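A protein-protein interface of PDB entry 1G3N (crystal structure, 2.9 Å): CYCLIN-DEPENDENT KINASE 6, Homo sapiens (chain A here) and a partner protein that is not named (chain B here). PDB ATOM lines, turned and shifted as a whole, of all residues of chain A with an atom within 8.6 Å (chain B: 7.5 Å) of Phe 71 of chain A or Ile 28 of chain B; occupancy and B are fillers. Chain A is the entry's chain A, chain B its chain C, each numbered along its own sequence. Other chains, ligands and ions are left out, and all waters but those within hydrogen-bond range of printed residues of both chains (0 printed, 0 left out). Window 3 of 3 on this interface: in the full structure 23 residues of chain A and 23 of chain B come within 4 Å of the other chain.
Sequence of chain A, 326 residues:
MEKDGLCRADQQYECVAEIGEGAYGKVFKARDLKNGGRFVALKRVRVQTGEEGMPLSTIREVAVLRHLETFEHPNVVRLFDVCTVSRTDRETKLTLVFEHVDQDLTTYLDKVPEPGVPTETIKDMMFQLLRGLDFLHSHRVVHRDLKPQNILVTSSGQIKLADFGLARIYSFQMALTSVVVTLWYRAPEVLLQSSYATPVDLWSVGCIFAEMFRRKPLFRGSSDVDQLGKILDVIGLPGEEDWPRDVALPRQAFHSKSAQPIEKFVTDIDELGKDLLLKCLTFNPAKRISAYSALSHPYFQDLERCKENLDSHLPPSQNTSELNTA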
ATOM      1  N   VAL A  64       0.394   5.458 -17.698  1.00  0.00           N
ATOM      2  CA  VAL A  64       1.020   6.571 -18.410  1.00  0.00           C
ATOM      3  C   VAL A  64       1.774   6.129 -19.672  1.00  0.00           C
ATOM      4  O   VAL A  64       1.744   6.800 -20.702  1.00  0.00           O
ATOM      5  CB  VAL A  64       1.994   7.326 -17.467  1.00  0.00           C
ATOM      6  CG1 VAL A  64       2.767   8.370 -18.232  1.00  0.00           C
ATOM      7  CG2 VAL A  64       1.213   7.951 -16.327  1.00  0.00           C
ATOM      8  N   LEU A  65       2.465   5.007 -19.588  1.00  0.00           N
ATOM      9  CA  LEU A  65       3.189   4.551 -20.752  1.00  0.00           C
ATOM     10  C   LEU A  65       2.180   4.241 -21.834  1.00  0.00           C
ATOM     11  O   LEU A  65       2.272   4.763 -22.945  1.00  0.00           O
ATOM     12  CB  LEU A  65       4.036   3.310 -20.411  1.00  0.00           C
ATOM     13  CG  LEU A  65       5.191   3.630 -19.443  1.00  0.00           C
ATOM     14  CD1 LEU A  65       5.877   2.351 -18.952  1.00  0.00           C
ATOM     15  CD2 LEU A  65       6.152   4.579 -20.177  1.00  0.00           C
ATOM     16  N   ARG A  66       1.209   3.399 -21.500  1.00  0.00           N
ATOM     17  CA  ARG A  66       0.166   3.034 -22.448  1.00  0.00           C
ATOM     18  C   ARG A  66      -0.475   4.275 -23.039  1.00  0.00           C
ATOM     19  O   ARG A  66      -0.757   4.341 -24.237  1.00  0.00           O
ATOM     20  CB  ARG A  66      -0.939   2.215 -21.757  1.00  0.00           C
ATOM     21  CG  ARG A  66      -0.691   0.729 -21.616  1.00  0.00           C
ATOM     22  CD  ARG A  66      -0.463   0.211 -22.991  1.00  0.00           C
ATOM     23  NE  ARG A  66      -0.825  -1.182 -23.186  1.00  0.00           N
ATOM     24  CZ  ARG A  66      -0.583  -1.827 -24.323  1.00  0.00           C
ATOM     25  NH1 ARG A  66       0.015  -1.178 -25.319  1.00  0.00           N
ATOM     26  NH2 ARG A  66      -0.928  -3.103 -24.475  1.00  0.00           N
ATOM     27  N   HIS A  67      -0.694   5.267 -22.192  1.00  0.00           N
ATOM     28  CA  HIS A  67      -1.358   6.436 -22.668  1.00  0.00           C
ATOM     29  C   HIS A  67      -0.545   7.315 -23.607  1.00  0.00           C
ATOM     30  O   HIS A  67      -1.078   7.788 -24.601  1.00  0.00           O
ATOM     31  CB  HIS A  67      -1.876   7.233 -21.485  1.00  0.00           C
ATOM     32  CG  HIS A  67      -2.951   8.189 -21.860  1.00  0.00           C
ATOM     33  ND1 HIS A  67      -4.198   7.762 -22.265  1.00  0.00           N
ATOM     34  CD2 HIS A  67      -2.931   9.530 -22.047  1.00  0.00           C
ATOM     35  CE1 HIS A  67      -4.896   8.802 -22.689  1.00  0.00           C
ATOM     36  NE2 HIS A  67      -4.150   9.886 -22.569  1.00  0.00           N
ATOM     37  N   LEU A  68       0.731   7.544 -23.298  1.00  0.00           N
ATOM     38  CA  LEU A  68       1.588   8.363 -24.137  1.00  0.00           C
ATOM     39  C   LEU A  68       1.804   7.668 -25.484  1.00  0.00           C
ATOM     40  O   LEU A  68       2.070   8.311 -26.509  1.00  0.00           O
ATOM     41  CB  LEU A  68       2.923   8.561 -23.454  1.00  0.00           C
ATOM     42  CG  LEU A  68       3.029   9.345 -22.149  1.00  0.00           C
ATOM     43  CD1 LEU A  68       4.436   9.153 -21.545  1.00  0.00           C
ATOM     44  CD2 LEU A  68       2.750  10.826 -22.430  1.00  0.00           C
ATOM     45  N   GLU A  69       1.695   6.343 -25.470  1.00  0.00           N
ATOM     46  CA  GLU A  69       1.873   5.540 -26.665  1.00  0.00           C
ATOM     47  C   GLU A  69       0.791   5.869 -27.697  1.00  0.00           C
ATOM     48  O   GLU A  69       1.033   5.824 -28.908  1.00  0.00           O
ATOM     49  CB  GLU A  69       1.818   4.071 -26.286  1.00  0.00           C
ATOM     50  CG  GLU A  69       1.648   3.150 -27.462  1.00  0.00           C
ATOM     51  CD  GLU A  69       2.807   3.209 -28.429  1.00  0.00           C
ATOM     52  OE1 GLU A  69       3.914   2.808 -28.015  1.00  0.00           O
ATOM     53  OE2 GLU A  69       2.628   3.652 -29.596  1.00  0.00           O
ATOM     54  N   THR A  70      -0.405   6.191 -27.205  1.00  0.00           N
ATOM     55  CA  THR A  70      -1.512   6.548 -28.061  1.00  0.00           C
ATOM     56  C   THR A  70      -1.053   7.580 -29.085  1.00  0.00           C
ATOM     57  O   THR A  70      -1.361   7.464 -30.275  1.00  0.00           O
ATOM     58  CB  THR A  70      -2.636   7.207 -27.274  1.00  0.00           C
ATOM     59  OG1 THR A  70      -2.749   6.595 -25.990  1.00  0.00           O
ATOM     60  CG2 THR A  70      -3.948   7.048 -28.018  1.00  0.00           C
ATOM     61  N   PHE A  71      -0.325   8.592 -28.606  1.00  0.00           N
ATOM     62  CA  PHE A  71       0.159   9.687 -29.461  1.00  0.00           C
ATOM     63  C   PHE A  71       1.229   9.313 -30.464  1.00  0.00           C
ATOM     64  O   PHE A  71       1.479  10.054 -31.396  1.00  0.00           O
ATOM     65  CB  PHE A  71       0.716  10.843 -28.628  1.00  0.00           C
ATOM     66  CG  PHE A  71      -0.234  11.384 -27.600  1.00  0.00           C
ATOM     67  CD1 PHE A  71      -0.428  10.718 -26.389  1.00  0.00           C
ATOM     68  CD2 PHE A  71      -0.901  12.576 -27.822  1.00  0.00           C
ATOM     69  CE1 PHE A  71      -1.274  11.242 -25.407  1.00  0.00           C
ATOM     70  CE2 PHE A  71      -1.739  13.097 -26.855  1.00  0.00           C
ATOM     71  CZ  PHE A  71      -1.930  12.431 -25.638  1.00  0.00           C
ATOM     72  N   GLU A  72       1.878   8.177 -30.258  1.00  0.00           N
ATOM     73  CA  GLU A  72       2.937   7.727 -31.156  1.00  0.00           C
ATOM     74  C   GLU A  72       3.968   8.789 -31.575  1.00  0.00           C
ATOM     75  O   GLU A  72       4.190   9.024 -32.764  1.00  0.00           O
ATOM     76  CB  GLU A  72       2.338   7.103 -32.412  1.00  0.00           C
ATOM     77  CG  GLU A  72       1.596   5.828 -32.176  1.00  0.00           C
ATOM     78  CD  GLU A  72       1.160   5.209 -33.475  1.00  0.00           C
ATOM     79  OE1 GLU A  72       0.407   5.889 -34.215  1.00  0.00           O
ATOM     80  OE2 GLU A  72       1.581   4.059 -33.757  1.00  0.00           O
ATOM     81  N   HIS A  73       4.613   9.421 -30.605  1.00  0.00           N
ATOM     82  CA  HIS A  73       5.619  10.399 -30.948  1.00  0.00           C
ATOM     83  C   HIS A  73       6.844   9.657 -31.490  1.00  0.00           C
ATOM     84  O   HIS A  73       7.321   8.682 -30.891  1.00  0.00           O
ATOM     85  CB  HIS A  73       6.021  11.215 -29.735  1.00  0.00           C
ATOM     86  CG  HIS A  73       6.842  12.425 -30.077  1.00  0.00           C
ATOM     87  ND1 HIS A  73       6.321  13.704 -30.083  1.00  0.00           N
ATOM     88  CD2 HIS A  73       8.144  12.548 -30.435  1.00  0.00           C
ATOM     89  CE1 HIS A  73       7.267  14.559 -30.422  1.00  0.00           C
ATOM     90  NE2 HIS A  73       8.383  13.882 -30.640  1.00  0.00           N
ATOM     91  N   PRO A  74       7.377  10.115 -32.637  1.00  0.00           N
ATOM     92  CA  PRO A  74       8.546   9.534 -33.318  1.00  0.00           C
ATOM     93  C   PRO A  74       9.850   9.567 -32.516  1.00  0.00           C
ATOM     94  O   PRO A  74      10.776   8.803 -32.766  1.00  0.00           O
ATOM     95  CB  PRO A  74       8.629  10.372 -34.591  1.00  0.00           C
ATOM     96  CG  PRO A  74       8.110  11.729 -34.103  1.00  0.00           C
ATOM     97  CD  PRO A  74       6.875  11.270 -33.406  1.00  0.00           C
ATOM     98  N   ASN A  75       9.900  10.444 -31.525  1.00  0.00           N
ATOM     99  CA  ASN A  75      11.095  10.601 -30.729  1.00  0.00           C
ATOM    100  C   ASN A  75      11.083   9.966 -29.342  1.00  0.00           C
ATOM    101  O   ASN A  75      11.917  10.268 -28.486  1.00  0.00           O
ATOM    102  CB  ASN A  75      11.418  12.092 -30.688  1.00  0.00           C
ATOM    103  CG  ASN A  75      11.653  12.644 -32.080  1.00  0.00           C
ATOM    104  OD1 ASN A  75      12.446  12.089 -32.836  1.00  0.00           O
ATOM    105  ND2 ASN A  75      10.965  13.713 -32.430  1.00  0.00           N
ATOM    106  N   VAL A  76      10.129   9.067 -29.144  1.00  0.00           N
ATOM    107  CA  VAL A  76       9.983   8.315 -27.909  1.00  0.00           C
ATOM    108  C   VAL A  76       9.913   6.848 -28.348  1.00  0.00           C
ATOM    109  O   VAL A  76       9.328   6.533 -29.399  1.00  0.00           O
ATOM    110  CB  VAL A  76       8.713   8.721 -27.167  1.00  0.00           C
ATOM    111  CG1 VAL A  76       8.571   7.884 -25.910  1.00  0.00           C
ATOM    112  CG2 VAL A  76       8.782  10.193 -26.812  1.00  0.00           C
ATOM    113  N   ARG A  78       8.741   3.159 -28.909  1.00  0.00           N
ATOM    114  CA  ARG A  78       7.422   2.512 -28.931  1.00  0.00           C
ATOM    115  C   ARG A  78       7.229   1.478 -27.847  1.00  0.00           C
ATOM    116  O   ARG A  78       8.152   0.746 -27.519  1.00  0.00           O
ATOM    117  CB  ARG A  78       7.155   1.776 -30.259  1.00  0.00           C
ATOM    118  CG  ARG A  78       6.618   2.581 -31.444  1.00  0.00           C
ATOM    119  CD  ARG A  78       5.507   3.529 -31.011  1.00  0.00           C
ATOM    120  NE  ARG A  78       6.078   4.828 -30.665  1.00  0.00           N
ATOM    121  CZ  ARG A  78       5.599   5.652 -29.744  1.00  0.00           C
ATOM    122  NH1 ARG A  78       6.206   6.811 -29.520  1.00  0.00           N
ATOM    123  NH2 ARG A  78       4.540   5.309 -29.029  1.00  0.00           N
ATOM    124  N   PHE A 135       7.485  16.775 -25.933  1.00  0.00           N
ATOM    125  CA  PHE A 135       6.299  15.936 -25.885  1.00  0.00           C
ATOM    126  C   PHE A 135       6.074  15.445 -24.457  1.00  0.00           C
ATOM    127  O   PHE A 135       5.007  15.626 -23.913  1.00  0.00           O
ATOM    128  CB  PHE A 135       6.432  14.774 -26.883  1.00  0.00           C
ATOM    129  CG  PHE A 135       5.370  13.707 -26.738  1.00  0.00           C
ATOM    130  CD1 PHE A 135       5.656  12.495 -26.088  1.00  0.00           C
ATOM    131  CD2 PHE A 135       4.081  13.912 -27.230  1.00  0.00           C
ATOM    132  CE1 PHE A 135       4.673  11.520 -25.938  1.00  0.00           C
ATOM    133  CE2 PHE A 135       3.092  12.939 -27.081  1.00  0.00           C
ATOM    134  CZ  PHE A 135       3.383  11.746 -26.438  1.00  0.00           C
ATOM    135  N   SER A 138       5.081  18.452 -22.003  1.00  0.00           N
ATOM    136  CA  SER A 138       3.737  18.921 -22.315  1.00  0.00           C
ATOM    137  C   SER A 138       2.644  17.990 -21.824  1.00  0.00           C
ATOM    138  O   SER A 138       1.491  18.391 -21.783  1.00  0.00           O
ATOM    139  CB  SER A 138       3.579  19.160 -23.814  1.00  0.00           C
ATOM    140  OG  SER A 138       3.607  17.944 -24.534  1.00  0.00           O
ATOM    141  N   HIS A 139       2.983  16.748 -21.473  1.00  0.00           N
ATOM    142  CA  HIS A 139       1.978  15.832 -20.923  1.00  0.00           C
ATOM    143  C   HIS A 139       2.287  15.563 -19.465  1.00  0.00           C
ATOM    144  O   HIS A 139       1.944  14.517 -18.916  1.00  0.00           O
ATOM    145  CB  HIS A 139       1.874  14.514 -21.694  1.00  0.00           C
ATOM    146  CG  HIS A 139       1.114  14.625 -22.978  1.00  0.00           C
ATOM    147  ND1 HIS A 139       1.667  15.126 -24.136  1.00  0.00           N
ATOM    148  CD2 HIS A 139      -0.182  14.364 -23.265  1.00  0.00           C
ATOM    149  CE1 HIS A 139       0.747  15.167 -25.083  1.00  0.00           C
ATOM    150  NE2 HIS A 139      -0.385  14.711 -24.580  1.00  0.00           N
ATOM    151  N   ARG B  20      -1.493  23.801 -27.814  1.00  0.00           N
ATOM    152  CA  ARG B  20      -0.923  22.657 -28.517  1.00  0.00           C
ATOM    153  C   ARG B  20      -1.245  21.306 -27.926  1.00  0.00           C
ATOM    154  O   ARG B  20      -1.433  20.342 -28.651  1.00  0.00           O
ATOM    155  CB  ARG B  20       0.586  22.824 -28.685  1.00  0.00           C
ATOM    156  CG  ARG B  20       0.880  23.565 -29.963  1.00  0.00           C
ATOM    157  CD  ARG B  20       0.244  22.779 -31.130  1.00  0.00           C
ATOM    158  NE  ARG B  20      -0.287  23.626 -32.206  1.00  0.00           N
ATOM    159  CZ  ARG B  20      -0.879  23.155 -33.304  1.00  0.00           C
ATOM    160  NH1 ARG B  20      -1.013  21.843 -33.475  1.00  0.00           N
ATOM    161  NH2 ARG B  20      -1.349  23.994 -34.223  1.00  0.00           N
ATOM    162  N   ILE B  21      -1.313  21.227 -26.610  1.00  0.00           N
ATOM    163  CA  ILE B  21      -1.653  19.966 -25.991  1.00  0.00           C
ATOM    164  C   ILE B  21      -3.084  19.666 -26.447  1.00  0.00           C
ATOM    165  O   ILE B  21      -3.363  18.583 -26.949  1.00  0.00           O
ATOM    166  CB  ILE B  21      -1.606  20.073 -24.458  1.00  0.00           C
ATOM    167  CG1 ILE B  21      -0.346  20.834 -24.028  1.00  0.00           C
ATOM    168  CG2 ILE B  21      -1.581  18.677 -23.848  1.00  0.00           C
ATOM    169  CD1 ILE B  21      -0.323  21.215 -22.546  1.00  0.00           C
ATOM    170  N   PHE B  22      -3.977  20.644 -26.289  1.00  0.00           N
ATOM    171  CA  PHE B  22      -5.380  20.504 -26.682  1.00  0.00           C
ATOM    172  C   PHE B  22      -5.468  19.892 -28.075  1.00  0.00           C
ATOM    173  O   PHE B  22      -6.012  18.804 -28.257  1.00  0.00           O
ATOM    174  CB  PHE B  22      -6.093  21.866 -26.673  1.00  0.00           C
ATOM    175  CG  PHE B  22      -7.592  21.785 -26.963  1.00  0.00           C
ATOM    176  CD1 PHE B  22      -8.477  21.214 -26.045  1.00  0.00           C
ATOM    177  CD2 PHE B  22      -8.113  22.254 -28.173  1.00  0.00           C
ATOM    178  CE1 PHE B  22      -9.841  21.112 -26.332  1.00  0.00           C
ATOM    179  CE2 PHE B  22      -9.473  22.151 -28.460  1.00  0.00           C
ATOM    180  CZ  PHE B  22     -10.333  21.580 -27.539  1.00  0.00           C
ATOM    181  N   TYR B  23      -4.932  20.595 -29.062  1.00  0.00           N
ATOM    182  CA  TYR B  23      -4.953  20.098 -30.424  1.00  0.00           C
ATOM    183  C   TYR B  23      -4.608  18.605 -30.527  1.00  0.00           C
ATOM    184  O   TYR B  23      -5.303  17.873 -31.234  1.00  0.00           O
ATOM    185  CB  TYR B  23      -3.993  20.913 -31.289  1.00  0.00           C
ATOM    186  CG  TYR B  23      -3.701  20.275 -32.632  1.00  0.00           C
ATOM    187  CD1 TYR B  23      -4.668  20.255 -33.649  1.00  0.00           C
ATOM    188  CD2 TYR B  23      -2.478  19.599 -32.855  1.00  0.00           C
ATOM    189  CE1 TYR B  23      -4.436  19.567 -34.858  1.00  0.00           C
ATOM    190  CE2 TYR B  23      -2.232  18.905 -34.056  1.00  0.00           C
ATOM    191  CZ  TYR B  23      -3.219  18.889 -35.050  1.00  0.00           C
ATOM    192  OH  TYR B  23      -3.002  18.158 -36.200  1.00  0.00           O
ATOM    193  N   ASN B  24      -3.551  18.147 -29.839  1.00  0.00           N
ATOM    194  CA  ASN B  24      -3.139  16.723 -29.891  1.00  0.00           C
ATOM    195  C   ASN B  24      -4.091  15.794 -29.152  1.00  0.00           C
ATOM    196  O   ASN B  24      -4.403  14.711 -29.632  1.00  0.00           O
ATOM    197  CB  ASN B  24      -1.736  16.500 -29.314  1.00  0.00           C
ATOM    198  CG  ASN B  24      -0.658  17.229 -30.082  1.00  0.00           C
ATOM    199  OD1 ASN B  24      -0.588  17.160 -31.321  1.00  0.00           O
ATOM    200  ND2 ASN B  24       0.214  17.922 -29.347  1.00  0.00           N
ATOM    201  N   ILE B  25      -4.527  16.219 -27.971  1.00  0.00           N
ATOM    202  CA  ILE B  25      -5.463  15.438 -27.195  1.00  0.00           C
ATOM    203  C   ILE B  25      -6.658  15.111 -28.100  1.00  0.00           C
ATOM    204  O   ILE B  25      -7.223  14.038 -28.032  1.00  0.00           O
ATOM    205  CB  ILE B  25      -5.966  16.230 -25.972  1.00  0.00           C
ATOM    206  CG1 ILE B  25      -4.785  16.774 -25.173  1.00  0.00           C
ATOM    207  CG2 ILE B  25      -6.840  15.346 -25.104  1.00  0.00           C
ATOM    208  CD1 ILE B  25      -3.826  15.727 -24.691  1.00  0.00           C
ATOM    209  N   LEU B  26      -7.023  16.043 -28.963  1.00  0.00           N
ATOM    210  CA  LEU B  26      -8.150  15.822 -29.841  1.00  0.00           C
ATOM    211  C   LEU B  26      -7.984  14.648 -30.797  1.00  0.00           C
ATOM    212  O   LEU B  26      -8.960  14.015 -31.185  1.00  0.00           O
ATOM    213  CB  LEU B  26      -8.460  17.087 -30.661  1.00  0.00           C
ATOM    214  CG  LEU B  26      -9.050  18.326 -29.977  1.00  0.00           C
ATOM    215  CD1 LEU B  26      -9.296  19.394 -31.021  1.00  0.00           C
ATOM    216  CD2 LEU B  26     -10.344  17.981 -29.280  1.00  0.00           C
ATOM    217  N   GLU B  27      -6.756  14.353 -31.194  1.00  0.00           N
ATOM    218  CA  GLU B  27      -6.542  13.257 -32.136  1.00  0.00           C
ATOM    219  C   GLU B  27      -6.656  11.914 -31.430  1.00  0.00           C
ATOM    220  O   GLU B  27      -7.190  10.955 -31.977  1.00  0.00           O
ATOM    221  CB  GLU B  27      -5.175  13.423 -32.803  1.00  0.00           C
ATOM    222  CG  GLU B  27      -5.022  14.796 -33.436  1.00  0.00           C
ATOM    223  CD  GLU B  27      -3.668  15.013 -34.070  1.00  0.00           C
ATOM    224  OE1 GLU B  27      -2.644  14.907 -33.352  1.00  0.00           O
ATOM    225  OE2 GLU B  27      -3.636  15.302 -35.290  1.00  0.00           O
ATOM    226  N   ILE B  28      -6.170  11.865 -30.197  1.00  0.00           N
ATOM    227  CA  ILE B  28      -6.218  10.665 -29.369  1.00  0.00           C
ATOM    228  C   ILE B  28      -7.669  10.326 -29.050  1.00  0.00           C
ATOM    229  O   ILE B  28      -8.131   9.224 -29.241  1.00  0.00           O
ATOM    230  CB  ILE B  28      -5.422  10.927 -28.058  1.00  0.00           C
ATOM    231  CG1 ILE B  28      -3.952  11.093 -28.421  1.00  0.00           C
ATOM    232  CG2 ILE B  28      -5.615   9.814 -27.041  1.00  0.00           C
ATOM    233  CD1 ILE B  28      -3.444  10.038 -29.369  1.00  0.00           C
ATOM    234  N   GLU B  29      -8.347  11.342 -28.560  1.00  0.00           N
ATOM    235  CA  GLU B  29      -9.730  11.348 -28.172  1.00  0.00           C
ATOM    236  C   GLU B  29     -10.598  10.175 -28.595  1.00  0.00           C
ATOM    237  O   GLU B  29     -11.034   9.397 -27.749  1.00  0.00           O
ATOM    238  CB  GLU B  29     -10.350  12.634 -28.684  1.00  0.00           C
ATOM    239  CG  GLU B  29     -11.149  13.414 -27.684  1.00  0.00           C
ATOM    240  CD  GLU B  29     -11.992  14.523 -28.340  1.00  0.00           C
ATOM    241  OE1 GLU B  29     -12.526  15.341 -27.572  1.00  0.00           O
ATOM    242  OE2 GLU B  29     -12.127  14.564 -29.598  1.00  0.00           O
ATOM    243  N   PRO B  30     -10.866  10.021 -29.909  1.00  0.00           N
ATOM    244  CA  PRO B  30     -11.718   8.918 -30.361  1.00  0.00           C
ATOM    245  C   PRO B  30     -11.375   7.564 -29.819  1.00  0.00           C
ATOM    246  O   PRO B  30     -12.233   6.715 -29.762  1.00  0.00           O
ATOM    247  CB  PRO B  30     -11.628   9.011 -31.884  1.00  0.00           C
ATOM    248  CG  PRO B  30     -10.349   9.693 -32.097  1.00  0.00           C
ATOM    249  CD  PRO B  30     -10.417  10.778 -31.076  1.00  0.00           C
ATOM    250  N   ARG B  31     -10.131   7.379 -29.404  1.00  0.00           N
ATOM    251  CA  ARG B  31      -9.668   6.127 -28.839  1.00  0.00           C
ATOM    252  C   ARG B  31     -10.402   5.706 -27.566  1.00  0.00           C
ATOM    253  O   ARG B  31     -10.325   4.555 -27.179  1.00  0.00           O
ATOM    254  CB  ARG B  31      -8.165   6.205 -28.521  1.00  0.00           C
ATOM    255  CG  ARG B  31      -7.343   5.218 -29.310  1.00  0.00           C
ATOM    256  CD  ARG B  31      -7.513   5.492 -30.835  1.00  0.00           C
ATOM    257  NE  ARG B  31      -6.615   6.518 -31.400  1.00  0.00           N
ATOM    258  CZ  ARG B  31      -6.893   7.264 -32.476  1.00  0.00           C
ATOM    259  NH1 ARG B  31      -8.047   7.128 -33.126  1.00  0.00           N
ATOM    260  NH2 ARG B  31      -5.990   8.125 -32.930  1.00  0.00           N
ATOM    261  N   PHE B  32     -11.110   6.611 -26.896  1.00  0.00           N
ATOM    262  CA  PHE B  32     -11.804   6.229 -25.665  1.00  0.00           C
ATOM    263  C   PHE B  32     -13.322   6.214 -25.742  1.00  0.00           C
ATOM    264  O   PHE B  32     -14.018   6.017 -24.740  1.00  0.00           O
ATOM    265  CB  PHE B  32     -11.295   7.102 -24.539  1.00  0.00           C
ATOM    266  CG  PHE B  32      -9.808   7.144 -24.501  1.00  0.00           C
ATOM    267  CD1 PHE B  32      -9.106   8.096 -25.247  1.00  0.00           C
ATOM    268  CD2 PHE B  32      -9.096   6.114 -23.883  1.00  0.00           C
ATOM    269  CE1 PHE B  32      -7.735   8.009 -25.382  1.00  0.00           C
ATOM    270  CE2 PHE B  32      -7.728   6.029 -24.017  1.00  0.00           C
ATOM    271  CZ  PHE B  32      -7.048   6.972 -24.767  1.00  0.00           C
ATOM    272  N   LEU B  33     -13.804   6.373 -26.967  1.00  0.00           N
ATOM    273  CA  LEU B  33     -15.204   6.351 -27.288  1.00  0.00           C
ATOM    274  C   LEU B  33     -15.803   4.977 -26.903  1.00  0.00           C
ATOM    275  O   LEU B  33     -15.165   3.954 -27.084  1.00  0.00           O
ATOM    276  CB  LEU B  33     -15.328   6.619 -28.791  1.00  0.00           C
ATOM    277  CG  LEU B  33     -16.166   7.817 -29.266  1.00  0.00           C
ATOM    278  CD1 LEU B  33     -16.275   8.894 -28.179  1.00  0.00           C
ATOM    279  CD2 LEU B  33     -15.520   8.354 -30.528  1.00  0.00           C
ATOM    280  N   ARG B 145      -4.312  -0.588 -19.893  1.00  0.00           N
ATOM    281  CA  ARG B 145      -4.616   0.685 -20.539  1.00  0.00           C
ATOM    282  C   ARG B 145      -5.754   1.277 -19.727  1.00  0.00           C
ATOM    283  O   ARG B 145      -6.903   1.200 -20.132  1.00  0.00           O
ATOM    284  CB  ARG B 145      -5.090   0.419 -21.944  1.00  0.00           C
ATOM    285  CG  ARG B 145      -4.940   1.609 -22.786  1.00  0.00           C
ATOM    286  CD  ARG B 145      -5.132   1.333 -24.247  1.00  0.00           C
ATOM    287  NE  ARG B 145      -4.578   2.415 -25.070  1.00  0.00           N
ATOM    288  CZ  ARG B 145      -4.517   3.723 -24.744  1.00  0.00           C
ATOM    289  NH1 ARG B 145      -4.969   4.210 -23.578  1.00  0.00           N
ATOM    290  NH2 ARG B 145      -4.021   4.587 -25.620  1.00  0.00           N
ATOM    291  N   ALA B 148      -7.523   7.499 -19.771  1.00  0.00           N
ATOM    292  CA  ALA B 148      -8.269   7.969 -20.928  1.00  0.00           C
ATOM    293  C   ALA B 148      -8.403   9.457 -20.856  1.00  0.00           C
ATOM    294  O   ALA B 148      -8.345  10.051 -19.769  1.00  0.00           O
ATOM    295  CB  ALA B 148      -9.667   7.354 -20.983  1.00  0.00           C
ATOM    296  N   VAL B 149      -8.534  10.065 -22.036  1.00  0.00           N
ATOM    297  CA  VAL B 149      -8.801  11.497 -22.122  1.00  0.00           C
ATOM    298  C   VAL B 149     -10.257  11.573 -21.621  1.00  0.00           C
ATOM    299  O   VAL B 149     -11.142  10.916 -22.170  1.00  0.00           O
ATOM    300  CB  VAL B 149      -8.820  11.998 -23.570  1.00  0.00           C
ATOM    301  CG1 VAL B 149      -9.426  13.409 -23.595  1.00  0.00           C
ATOM    302  CG2 VAL B 149      -7.423  11.938 -24.182  1.00  0.00           C
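OG1 of Thr 70 of chain A sits at hydrogen-bond distance from NH2 of Arg 145 of chain B (2.4 Å).
The backbone carbonyl oxygen (O) of His 67 of chain A sits at hydrogen-bond distance from the side-chain hydroxyl (OG1) of Thr 70 of chain A, at 2.5 Å.
The side-chain hydroxyl (OG) of Ser 138 of chain A is in hydrogen-bond range of the backbone carbonyl oxygen (O) of Phe 135 of chain A.
The backbone carbonyl oxygen (O) of Phe 135 of chain A is in hydrogen-bond range of a ring nitrogen (ND1) of His 139 of chain A, 3.4 Å away.
OG of Ser 138 of chain A is in hydrogen-bond range of ND1 of His 139 of chain A (3.4 Å).
Among the printed residues, pairs that only touch across the chains: Thr 70 of chain A with Ile 28 of chain B (3.3 Å), Phe 71 of chain A with Ile 28 of chain B (3.4 Å), Ser 138 of chain A with Ile 21 of chain B (3.4 Å), His 67 of chain A with Phe 32 of chain B (3.5 Å), Arg 66 of chain A with Arg 145 of chain B (3.6 Å), His 139 of chain A with Ile 25 of chain B (3.6 Å), His 67 of chain A with Arg 145 of chain B (3.9 Å), His 67 of chain A with Ala 148 of chain B (3.9 Å), His 67 of chain A with Val 149 of chain B (3.9 Å) and Phe 71 of chain A with Ile 25 of chain B (3.9 Å).
Of the printed residues of chain B, Arg 66 of chain A touches Arg 145 (3.6 Å).
Of the printed residues of chain B, His 67 of chain A touches Phe 32 (3.5 Å), Arg 145 (3.9 Å), Ala 148 (3.9 Å) and Val 149 (3.9 Å).
Of the printed residues of chain B, Thr 70 of chain A touches Ile 28 and Arg 145.
Printed residues of chain B within 4 Å of Phe 71 of chain A: Ile 25 (3.9 Å) and Ile 28 (3.4 Å).
Glu 27 of chain B touches none of the printed residues of chain A.
Ile 28 of chain B touches just these residues of chain A: Thr 70 (3.3 Å) and Phe 71 (3.4 Å).
Printed residues of chain A within 4 Å of Phe 32 of chain B: His 67.
Printed residues of chain A within 4 Å of Ala 148 of chain B: His 67 (3.9 Å).
The nearest residue of chain B that does not touch Phe 71 of chain A is Asn 24 of chain B (4.2 Å).
The nearest residue of chain A that does not touch Ile 28 of chain B is His 67 of chain A (4.5 Å).
The nearest printed residue of chain B that does not touch Ser 138 of chain A is Asn 24 of chain B (5.9 Å).
Printed residues of chain A that touch a printed residue of chain B: Arg 66, His 67, Thr 70, Phe 71, Ser 138 and His 139.
Printed residues of chain B that touch a printed residue of chain A: Ile 21, Ile 25, Ile 28, Phe 32, Arg 145, Ala 148 and Val 149.
Hydrophobic or aromatic side chains of chain B within 4 Å of the printed part of chain A: Ile 21, Ile 25, Ile 28 and Phe 32.
Among the printed residues, 11 pairs touch across the chains.
Among the printed residues, no Asp or Glu carboxylate lies within 4 Å of a Lys or Arg side-chain nitrogen of the other chain.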
